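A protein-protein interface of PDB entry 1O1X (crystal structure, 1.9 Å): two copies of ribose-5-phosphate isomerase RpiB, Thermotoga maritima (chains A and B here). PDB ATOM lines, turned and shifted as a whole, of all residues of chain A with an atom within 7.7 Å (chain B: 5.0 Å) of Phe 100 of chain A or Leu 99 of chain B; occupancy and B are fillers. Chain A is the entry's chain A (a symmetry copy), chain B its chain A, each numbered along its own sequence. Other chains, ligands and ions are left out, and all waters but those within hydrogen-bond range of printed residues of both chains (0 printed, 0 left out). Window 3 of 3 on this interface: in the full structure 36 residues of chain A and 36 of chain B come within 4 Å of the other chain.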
ATOM      1  N   LEU A  81      24.724  25.884  11.688  1.00  0.00           N
ATOM      2  CA  LEU A  81      24.614  25.197  12.972  1.00  0.00           C
ATOM      3  C   LEU A  81      24.274  26.153  14.116  1.00  0.00           C
ATOM      4  O   LEU A  81      23.361  25.884  14.884  1.00  0.00           O
ATOM      5  CB  LEU A  81      25.880  24.421  13.257  1.00  0.00           C
ATOM      6  CG  LEU A  81      26.131  23.242  12.273  1.00  0.00           C
ATOM      7  CD1 LEU A  81      27.485  22.666  12.521  1.00  0.00           C
ATOM      8  CD2 LEU A  81      25.077  22.195  12.373  1.00  0.00           C
ATOM      9  N   LEU A  97      17.474  23.555   9.557  1.00  0.00           N
ATOM     10  CA  LEU A  97      18.709  23.647   8.772  1.00  0.00           C
ATOM     11  C   LEU A  97      18.552  22.712   7.556  1.00  0.00           C
ATOM     12  O   LEU A  97      18.520  21.474   7.701  1.00  0.00           O
ATOM     13  CB  LEU A  97      19.887  23.237   9.659  1.00  0.00           C
ATOM     14  CG  LEU A  97      21.283  23.191   9.043  1.00  0.00           C
ATOM     15  CD1 LEU A  97      21.574  24.420   8.259  1.00  0.00           C
ATOM     16  CD2 LEU A  97      22.375  22.929  10.097  1.00  0.00           C
ATOM     17  N   CYS A  98      18.421  23.290   6.372  1.00  0.00           N
ATOM     18  CA  CYS A  98      18.161  22.533   5.156  1.00  0.00           C
ATOM     19  C   CYS A  98      19.263  22.747   4.149  1.00  0.00           C
ATOM     20  O   CYS A  98      19.575  23.899   3.785  1.00  0.00           O
ATOM     21  CB  CYS A  98      16.824  22.967   4.555  1.00  0.00           C
ATOM     22  SG  CYS A  98      15.381  22.713   5.634  1.00  0.00           S
ATOM     23  N   LEU A  99      19.850  21.650   3.690  1.00  0.00           N
ATOM     24  CA  LEU A  99      20.956  21.717   2.727  1.00  0.00           C
ATOM     25  C   LEU A  99      20.538  21.411   1.297  1.00  0.00           C
ATOM     26  O   LEU A  99      21.318  21.570   0.352  1.00  0.00           O
ATOM     27  CB  LEU A  99      22.081  20.778   3.145  1.00  0.00           C
ATOM     28  CG  LEU A  99      23.220  21.509   3.856  1.00  0.00           C
ATOM     29  CD1 LEU A  99      22.706  22.128   5.167  1.00  0.00           C
ATOM     30  CD2 LEU A  99      24.397  20.539   4.099  1.00  0.00           C
ATOM     31  N   PHE A 100      19.333  20.882   1.132  1.00  0.00           N
ATOM     32  CA  PHE A 100      18.765  20.637  -0.209  1.00  0.00           C
ATOM     33  C   PHE A 100      17.206  20.682  -0.126  1.00  0.00           C
ATOM     34  O   PHE A 100      16.642  20.591   0.987  1.00  0.00           O
ATOM     35  CB  PHE A 100      19.323  19.349  -0.888  1.00  0.00           C
ATOM     36  CG  PHE A 100      19.141  18.075  -0.081  1.00  0.00           C
ATOM     37  CD1 PHE A 100      20.077  17.698   0.865  1.00  0.00           C
ATOM     38  CD2 PHE A 100      18.040  17.241  -0.299  1.00  0.00           C
ATOM     39  CE1 PHE A 100      19.904  16.523   1.602  1.00  0.00           C
ATOM     40  CE2 PHE A 100      17.878  16.093   0.405  1.00  0.00           C
ATOM     41  CZ  PHE A 100      18.785  15.740   1.368  1.00  0.00           C
ATOM     42  N   PRO A 101      16.528  20.900  -1.257  1.00  0.00           N
ATOM     43  CA  PRO A 101      15.078  21.148  -1.247  1.00  0.00           C
ATOM     44  C   PRO A 101      14.192  20.132  -0.541  1.00  0.00           C
ATOM     45  O   PRO A 101      13.251  20.555   0.149  1.00  0.00           O
ATOM     46  CB  PRO A 101      14.759  21.303  -2.720  1.00  0.00           C
ATOM     47  CG  PRO A 101      16.041  21.893  -3.288  1.00  0.00           C
ATOM     48  CD  PRO A 101      17.081  21.080  -2.620  1.00  0.00           C
ATOM     49  N   ASP A 102      14.455  18.843  -0.669  1.00  0.00           N
ATOM     50  CA  ASP A 102      13.666  17.850   0.064  1.00  0.00           C
ATOM     51  C   ASP A 102      13.710  18.013   1.560  1.00  0.00           C
ATOM     52  O   ASP A 102      12.731  17.684   2.248  1.00  0.00           O
ATOM     53  CB  ASP A 102      14.054  16.430  -0.281  1.00  0.00           C
ATOM     54  CG  ASP A 102      13.661  16.065  -1.694  1.00  0.00           C
ATOM     55  OD1 ASP A 102      14.416  16.451  -2.622  1.00  0.00           O
ATOM     56  OD2 ASP A 102      12.597  15.460  -1.955  1.00  0.00           O
ATOM     57  N   MET A 103      14.809  18.534   2.101  1.00  0.00           N
ATOM     58  CA  MET A 103      14.824  18.807   3.514  1.00  0.00           C
ATOM     59  C   MET A 103      13.837  19.914   3.901  1.00  0.00           C
ATOM     60  O   MET A 103      13.153  19.801   4.932  1.00  0.00           O
ATOM     61  CB  MET A 103      16.246  19.114   3.991  1.00  0.00           C
ATOM     62  CG  MET A 103      17.145  17.912   3.932  1.00  0.00           C
ATOM     63  SD  MET A 103      18.927  18.287   4.736  1.00  0.00           S
ATOM     64  CE  MET A 103      18.440  18.295   6.619  1.00  0.00           C
ATOM     65  N   ALA A 104      13.767  20.967   3.085  1.00  0.00           N
ATOM     66  CA  ALA A 104      12.827  22.046   3.298  1.00  0.00           C
ATOM     67  C   ALA A 104      11.408  21.534   3.133  1.00  0.00           C
ATOM     68  O   ALA A 104      10.521  21.950   3.878  1.00  0.00           O
ATOM     69  CB  ALA A 104      13.070  23.213   2.330  1.00  0.00           C
ATOM     70  N   ARG A 105      11.180  20.667   2.147  1.00  0.00           N
ATOM     71  CA  ARG A 105       9.866  20.073   1.963  1.00  0.00           C
ATOM     72  C   ARG A 105       9.424  19.354   3.261  1.00  0.00           C
ATOM     73  O   ARG A 105       8.344  19.581   3.759  1.00  0.00           O
ATOM     74  CB  ARG A 105       9.849  19.123   0.756  1.00  0.00           C
ATOM     75  CG  ARG A 105       8.567  18.292   0.604  1.00  0.00           C
ATOM     76  CD  ARG A 105       8.600  17.379  -0.589  1.00  0.00           C
ATOM     77  NE  ARG A 105       9.649  16.344  -0.503  1.00  0.00           N
ATOM     78  CZ  ARG A 105       9.577  15.183   0.191  1.00  0.00           C
ATOM     79  NH1 ARG A 105       8.501  14.885   0.909  1.00  0.00           N
ATOM     80  NH2 ARG A 105      10.598  14.311   0.157  1.00  0.00           N
ATOM     81  N   LEU A 106      10.270  18.485   3.794  1.00  0.00           N
ATOM     82  CA  LEU A 106       9.938  17.748   4.988  1.00  0.00           C
ATOM     83  C   LEU A 106       9.880  18.649   6.232  1.00  0.00           C
ATOM     84  O   LEU A 106       9.042  18.454   7.083  1.00  0.00           O
ATOM     85  CB  LEU A 106      10.893  16.550   5.172  1.00  0.00           C
ATOM     86  CG  LEU A 106      10.693  15.390   4.174  1.00  0.00           C
ATOM     87  CD1 LEU A 106      11.752  14.365   4.297  1.00  0.00           C
ATOM     88  CD2 LEU A 106       9.341  14.762   4.342  1.00  0.00           C
ATOM     89  N   LEU A 116      13.573  28.850   8.277  1.00  0.00           N
ATOM     90  CA  LEU A 116      14.501  28.142   7.414  1.00  0.00           C
ATOM     91  C   LEU A 116      15.921  28.607   7.761  1.00  0.00           C
ATOM     92  O   LEU A 116      16.196  29.787   7.781  1.00  0.00           O
ATOM     93  CB  LEU A 116      14.206  28.427   5.942  1.00  0.00           C
ATOM     94  CG  LEU A 116      15.271  28.021   4.910  1.00  0.00           C
ATOM     95  CD1 LEU A 116      15.411  26.524   4.940  1.00  0.00           C
ATOM     96  CD2 LEU A 116      14.902  28.509   3.533  1.00  0.00           C
ATOM     97  N   LEU A 118      19.898  28.361   6.606  1.00  0.00           N
ATOM     98  CA  LEU A 118      20.765  28.069   5.494  1.00  0.00           C
ATOM     99  C   LEU A 118      22.230  28.282   5.850  1.00  0.00           C
ATOM    100  O   LEU A 118      22.575  29.217   6.544  1.00  0.00           O
ATOM    101  CB  LEU A 118      20.443  28.984   4.306  1.00  0.00           C
ATOM    102  CG  LEU A 118      19.046  28.917   3.736  1.00  0.00           C
ATOM    103  CD1 LEU A 118      18.799  30.075   2.778  1.00  0.00           C
ATOM    104  CD2 LEU A 118      18.840  27.593   3.042  1.00  0.00           C
ATOM    105  N   PRO A 119      23.088  27.414   5.339  1.00  0.00           N
ATOM    106  CA  PRO A 119      24.528  27.563   5.500  1.00  0.00           C
ATOM    107  C   PRO A 119      25.203  28.437   4.425  1.00  0.00           C
ATOM    108  O   PRO A 119      25.504  27.971   3.296  1.00  0.00           O
ATOM    109  CB  PRO A 119      25.020  26.152   5.381  1.00  0.00           C
ATOM    110  CG  PRO A 119      24.099  25.524   4.453  1.00  0.00           C
ATOM    111  CD  PRO A 119      22.750  26.190   4.616  1.00  0.00           C
ATOM    112  N   ILE A 123      26.542  26.261   0.750  1.00  0.00           N
ATOM    113  CA  ILE A 123      25.732  26.088  -0.437  1.00  0.00           C
ATOM    114  C   ILE A 123      25.818  27.269  -1.391  1.00  0.00           C
ATOM    115  O   ILE A 123      26.105  28.402  -1.020  1.00  0.00           O
ATOM    116  CB  ILE A 123      24.229  25.779  -0.150  1.00  0.00           C
ATOM    117  CG1 ILE A 123      23.549  26.930   0.582  1.00  0.00           C
ATOM    118  CG2 ILE A 123      24.076  24.424   0.569  1.00  0.00           C
ATOM    119  CD1 ILE A 123      21.987  26.693   0.638  1.00  0.00           C
ATOM    120  N   LEU A 127      21.065  26.906  -5.462  1.00  0.00           N
ATOM    121  CA  LEU A 127      20.512  25.863  -4.590  1.00  0.00           C
ATOM    122  C   LEU A 127      19.710  26.445  -3.436  1.00  0.00           C
ATOM    123  O   LEU A 127      18.631  25.925  -3.089  1.00  0.00           O
ATOM    124  CB  LEU A 127      21.607  24.942  -4.075  1.00  0.00           C
ATOM    125  CG  LEU A 127      21.202  23.813  -3.122  1.00  0.00           C
ATOM    126  CD1 LEU A 127      20.215  22.909  -3.814  1.00  0.00           C
ATOM    127  CD2 LEU A 127      22.419  23.000  -2.671  1.00  0.00           C
ATOM    128  N   ALA A 128      20.250  27.478  -2.794  1.00  0.00           N
ATOM    129  CA  ALA A 128      19.536  28.207  -1.726  1.00  0.00           C
ATOM    130  C   ALA A 128      18.172  28.698  -2.209  1.00  0.00           C
ATOM    131  O   ALA A 128      17.200  28.599  -1.502  1.00  0.00           O
ATOM    132  CB  ALA A 128      20.369  29.407  -1.260  1.00  0.00           C
ATOM    133  N   TRP A 130      16.242  27.429  -4.602  1.00  0.00           N
ATOM    134  CA  TRP A 130      15.364  26.281  -4.691  1.00  0.00           C
ATOM    135  C   TRP A 130      14.872  25.829  -3.325  1.00  0.00           C
ATOM    136  O   TRP A 130      13.701  25.425  -3.190  1.00  0.00           O
ATOM    137  CB  TRP A 130      16.013  25.055  -5.350  1.00  0.00           C
ATOM    138  CG  TRP A 130      16.554  25.271  -6.709  1.00  0.00           C
ATOM    139  CD1 TRP A 130      16.229  26.249  -7.594  1.00  0.00           C
ATOM    140  CD2 TRP A 130      17.561  24.464  -7.341  1.00  0.00           C
ATOM    141  NE1 TRP A 130      17.020  26.127  -8.718  1.00  0.00           N
ATOM    142  CE2 TRP A 130      17.851  25.047  -8.577  1.00  0.00           C
ATOM    143  CE3 TRP A 130      18.289  23.348  -6.943  1.00  0.00           C
ATOM    144  CZ2 TRP A 130      18.822  24.528  -9.445  1.00  0.00           C
ATOM    145  CZ3 TRP A 130      19.235  22.812  -7.805  1.00  0.00           C
ATOM    146  CH2 TRP A 130      19.501  23.412  -9.034  1.00  0.00           C
ATOM    147  N   ILE A 131      15.750  25.872  -2.326  1.00  0.00           N
ATOM    148  CA  ILE A 131      15.377  25.489  -0.961  1.00  0.00           C
ATOM    149  C   ILE A 131      14.331  26.462  -0.427  1.00  0.00           C
ATOM    150  O   ILE A 131      13.306  26.041   0.146  1.00  0.00           O
ATOM    151  CB  ILE A 131      16.621  25.402  -0.025  1.00  0.00           C
ATOM    152  CG1 ILE A 131      17.570  24.274  -0.478  1.00  0.00           C
ATOM    153  CG2 ILE A 131      16.239  25.186   1.431  1.00  0.00           C
ATOM    154  CD1 ILE A 131      18.944  24.352   0.162  1.00  0.00           C
ATOM    155  N   VAL A 132      14.565  27.746  -0.640  1.00  0.00           N
ATOM    156  CA  VAL A 132      13.638  28.803  -0.214  1.00  0.00           C
ATOM    157  C   VAL A 132      12.265  28.635  -0.878  1.00  0.00           C
ATOM    158  O   VAL A 132      11.246  28.710  -0.199  1.00  0.00           O
ATOM    159  CB  VAL A 132      14.220  30.211  -0.506  1.00  0.00           C
ATOM    160  CG1 VAL A 132      13.147  31.305  -0.373  1.00  0.00           C
ATOM    161  CG2 VAL A 132      15.402  30.518   0.400  1.00  0.00           C
ATOM    162  N   THR A 134      10.888  25.943  -2.112  1.00  0.00           N
ATOM    163  CA  THR A 134      10.251  24.751  -1.533  1.00  0.00           C
ATOM    164  C   THR A 134       9.676  25.022  -0.129  1.00  0.00           C
ATOM    165  O   THR A 134       8.532  24.659   0.188  1.00  0.00           O
ATOM    166  CB  THR A 134      11.285  23.633  -1.466  1.00  0.00           C
ATOM    167  OG1 THR A 134      11.730  23.351  -2.794  1.00  0.00           O
ATOM    168  CG2 THR A 134      10.675  22.342  -0.949  1.00  0.00           C
ATOM    169  N   LEU B  97      23.069  19.200  13.666  1.00  0.00           N
ATOM    170  CA  LEU B  97      22.645  18.353  12.546  1.00  0.00           C
ATOM    171  C   LEU B  97      23.769  18.389  11.491  1.00  0.00           C
ATOM    172  O   LEU B  97      24.012  19.431  10.850  1.00  0.00           O
ATOM    173  CB  LEU B  97      21.325  18.895  11.992  1.00  0.00           C
ATOM    174  CG  LEU B  97      20.711  18.214  10.772  1.00  0.00           C
ATOM    175  CD1 LEU B  97      20.688  16.736  10.927  1.00  0.00           C
ATOM    176  CD2 LEU B  97      19.310  18.763  10.443  1.00  0.00           C
ATOM    177  N   CYS B  98      24.473  17.278  11.332  1.00  0.00           N
ATOM    178  CA  CYS B  98      25.627  17.203  10.448  1.00  0.00           C
ATOM    179  C   CYS B  98      25.410  16.165   9.376  1.00  0.00           C
ATOM    180  O   CYS B  98      25.124  14.989   9.680  1.00  0.00           O
ATOM    181  CB  CYS B  98      26.874  16.852  11.259  1.00  0.00           C
ATOM    182  SG  CYS B  98      27.303  18.050  12.560  1.00  0.00           S
ATOM    183  N   LEU B  99      25.552  16.585   8.125  1.00  0.00           N
ATOM    184  CA  LEU B  99      25.340  15.685   6.985  1.00  0.00           C
ATOM    185  C   LEU B  99      26.633  15.177   6.364  1.00  0.00           C
ATOM    186  O   LEU B  99      26.625  14.299   5.494  1.00  0.00           O
ATOM    187  CB  LEU B  99      24.492  16.367   5.920  1.00  0.00           C
ATOM    188  CG  LEU B  99      23.024  15.941   5.980  1.00  0.00           C
ATOM    189  CD1 LEU B  99      22.409  16.373   7.321  1.00  0.00           C
ATOM    190  CD2 LEU B  99      22.257  16.530   4.776  1.00  0.00           C
ATOM    191  N   PHE B 100      27.750  15.789   6.736  1.00  0.00           N
ATOM    192  CA  PHE B 100      29.079  15.325   6.289  1.00  0.00           C
ATOM    193  C   PHE B 100      30.151  15.733   7.349  1.00  0.00           C
ATOM    194  O   PHE B 100      29.877  16.603   8.204  1.00  0.00           O
ATOM    195  CB  PHE B 100      29.429  15.768   4.835  1.00  0.00           C
ATOM    196  CG  PHE B 100      29.370  17.267   4.596  1.00  0.00           C
ATOM    197  CD1 PHE B 100      28.181  17.879   4.244  1.00  0.00           C
ATOM    198  CD2 PHE B 100      30.521  18.053   4.695  1.00  0.00           C
ATOM    199  CE1 PHE B 100      28.134  19.259   4.023  1.00  0.00           C
ATOM    200  CE2 PHE B 100      30.481  19.389   4.466  1.00  0.00           C
ATOM    201  CZ  PHE B 100      29.296  20.001   4.156  1.00  0.00           C
ATOM    202  N   PRO B 101      31.310  15.067   7.351  1.00  0.00           N
ATOM    203  CA  PRO B 101      32.298  15.249   8.425  1.00  0.00           C
ATOM    204  C   PRO B 101      32.752  16.668   8.737  1.00  0.00           C
ATOM    205  O   PRO B 101      32.891  16.991   9.927  1.00  0.00           O
ATOM    206  CB  PRO B 101      33.429  14.339   7.992  1.00  0.00           C
ATOM    207  CG  PRO B 101      32.707  13.227   7.245  1.00  0.00           C
ATOM    208  CD  PRO B 101      31.729  13.982   6.431  1.00  0.00           C
ATOM    209  N   MET B 103      31.023  19.300   8.703  1.00  0.00           N
ATOM    210  CA  MET B 103      30.043  19.924   9.554  1.00  0.00           C
ATOM    211  C   MET B 103      30.238  19.555  11.029  1.00  0.00           C
ATOM    212  O   MET B 103      30.109  20.425  11.907  1.00  0.00           O
ATOM    213  CB  MET B 103      28.626  19.614   9.067  1.00  0.00           C
ATOM    214  CG  MET B 103      28.312  20.271   7.754  1.00  0.00           C
ATOM    215  SD  MET B 103      26.407  20.011   7.238  1.00  0.00           S
ATOM    216  CE  MET B 103      25.561  21.243   8.484  1.00  0.00           C
ATOM    217  N   PRO B 119      20.688  12.333  10.293  1.00  0.00           N
ATOM    218  CA  PRO B 119      19.498  11.951   9.544  1.00  0.00           C
ATOM    219  C   PRO B 119      19.470  10.476   9.101  1.00  0.00           C
ATOM    220  O   PRO B 119      20.086  10.088   8.076  1.00  0.00           O
ATOM    221  CB  PRO B 119      19.570  12.837   8.337  1.00  0.00           C
ATOM    222  CG  PRO B 119      20.991  13.000   8.093  1.00  0.00           C
ATOM    223  CD  PRO B 119      21.703  12.927   9.426  1.00  0.00           C
ATOM    224  N   LEU B 122      18.552   9.680   5.392  1.00  0.00           N
ATOM    225  CA  LEU B 122      19.191  10.468   4.372  1.00  0.00           C
ATOM    226  C   LEU B 122      20.642  10.036   4.107  1.00  0.00           C
ATOM    227  O   LEU B 122      21.084  10.110   2.969  1.00  0.00           O
ATOM    228  CB  LEU B 122      19.171  11.942   4.717  1.00  0.00           C
ATOM    229  CG  LEU B 122      17.811  12.622   4.900  1.00  0.00           C
ATOM    230  CD1 LEU B 122      18.074  14.087   5.151  1.00  0.00           C
ATOM    231  CD2 LEU B 122      16.866  12.420   3.764  1.00  0.00           C
ATOM    232  N   ILE B 123      21.381   9.627   5.144  1.00  0.00           N
ATOM    233  CA  ILE B 123      22.771   9.261   4.971  1.00  0.00           C
ATOM    234  C   ILE B 123      23.018   7.770   5.143  1.00  0.00           C
ATOM    235  O   ILE B 123      22.287   7.051   5.815  1.00  0.00           O
ATOM    236  CB  ILE B 123      23.762  10.046   5.885  1.00  0.00           C
ATOM    237  CG1 ILE B 123      23.501   9.771   7.362  1.00  0.00           C
ATOM    238  CG2 ILE B 123      23.757  11.547   5.536  1.00  0.00           C
ATOM    239  CD1 ILE B 123      24.664  10.379   8.243  1.00  0.00           C
ATOM    240  N   LEU B 127      29.164   6.837   5.941  1.00  0.00           N
ATOM    241  CA  LEU B 127      29.275   8.290   6.107  1.00  0.00           C
ATOM    242  C   LEU B 127      28.979   8.731   7.532  1.00  0.00           C
ATOM    243  O   LEU B 127      29.676   9.606   8.083  1.00  0.00           O
ATOM    244  CB  LEU B 127      28.382   9.024   5.119  1.00  0.00           C
ATOM    245  CG  LEU B 127      28.355  10.554   5.180  1.00  0.00           C
ATOM    246  CD1 LEU B 127      29.743  11.086   4.930  1.00  0.00           C
ATOM    247  CD2 LEU B 127      27.386  11.137   4.147  1.00  0.00           C
ATOM    248  N   ILE B 131      31.304  10.825  10.262  1.00  0.00           N
ATOM    249  CA  ILE B 131      30.803  12.021  10.947  1.00  0.00           C
ATOM    250  C   ILE B 131      30.981  11.856  12.453  1.00  0.00           C
ATOM    251  O   ILE B 131      31.470  12.776  13.139  1.00  0.00           O
ATOM    252  CB  ILE B 131      29.323  12.328  10.566  1.00  0.00           C
ATOM    253  CG1 ILE B 131      29.204  12.683   9.071  1.00  0.00           C
ATOM    254  CG2 ILE B 131      28.729  13.451  11.401  1.00  0.00           C
ATOM    255  CD1 ILE B 131      27.775  12.656   8.559  1.00  0.00           C
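The side-chain sulfur of Cys 98 of chain A lies close to the backbone carbonyl oxygen of Met 103 of chain A, at 3.7 Å.
SG of Cys 98 of chain B lies close to O of Met 103 of chain B (3.7 Å).
N of Leu 99 of chain B sits at hydrogen-bond distance from SD of Met 103 of chain B (3.6 Å).
The side-chain sulfur of Met 103 of chain A sits at hydrogen-bond distance from the backbone NH of Leu 99 of chain A, at 3.6 Å.
Among the printed residues, pairs that only touch across the chains: Leu 81 of chain A with Leu 97 of chain B (3.3 Å), Leu 81 of chain A with Met 103 of chain B (3.5 Å), Leu 97 of chain A with Leu 97 of chain B (3.9 Å), Leu 97 of chain A with Met 103 of chain B (3.9 Å), Leu 99 of chain A with Phe 100 of chain B (3.95 Å), Leu 99 of chain A with Met 103 of chain B (3.8 Å), Phe 100 of chain A with Leu 99 of chain B (3.95 Å), Met 103 of chain A with Leu 97 of chain B (3.9 Å) and Met 103 of chain A with Leu 99 of chain B (3.8 Å).
Printed residues of chain B within 4 Å of Phe 100 of chain A: Leu 99.
Printed residues of chain A within 4 Å of Leu 99 of chain B: Phe 100 (3.95 Å) and Met 103 (3.8 Å).
Of the printed residues of chain B, Leu 97 of chain A touches Leu 97 and Met 103.
Printed residues of chain B within 4 Å of Leu 81 of chain A: Leu 97 and Met 103.
Printed residues of chain B within 4 Å of Met 103 of chain A: Leu 97 (3.9 Å) and Leu 99 (3.8 Å).
Of the printed residues of chain A, Phe 100 of chain B touches Leu 99.
Of the printed residues of chain B, Leu 99 of chain A touches Phe 100 and Met 103.
The nearest printed residue of chain B that does not touch Phe 100 of chain A is Leu 122 of chain B (4.2 Å).
Of the 11 printed residues of chain B, 4 touch a printed residue of chain A.
Hydrophobic or aromatic side chains of chain B within 4 Å of the printed part of chain A: Leu 97, Leu 99, Phe 100 and Met 103.
Along chain B the printed residues that touch a printed residue of chain A span positions 97 to 103.
Hydrophobic or aromatic side chains of chain A that line the printed part of chain B: Leu 81, Leu 97, Leu 99, Phe 100 and Met 103.
Along chain A the printed residues that touch a printed residue of chain B span positions 81 to 103.
Among the printed residues, 9 pairs touch across the chains.
Among the printed residues, no Asp or Glu carboxylate lies within 4 Å of a Lys or Arg side-chain nitrogen of the other chain.
Leu 97 of chain B touches its own counterpart, Leu 97 of chain A.
Leu 97 of chain A touches Met 103 of chain B, and with the chains exchanged Met 103 of chain A touches Leu 97 of chain B.
Leu 99 of chain A touches Phe 100 of chain B, and with the chains exchanged Phe 100 of chain A touches Leu 99 of chain B.
Leu 99 of chain A touches Met 103 of chain B, and with the chains exchanged Met 103 of chain A touches Leu 99 of chain B.
10 positions are printed for both chains.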
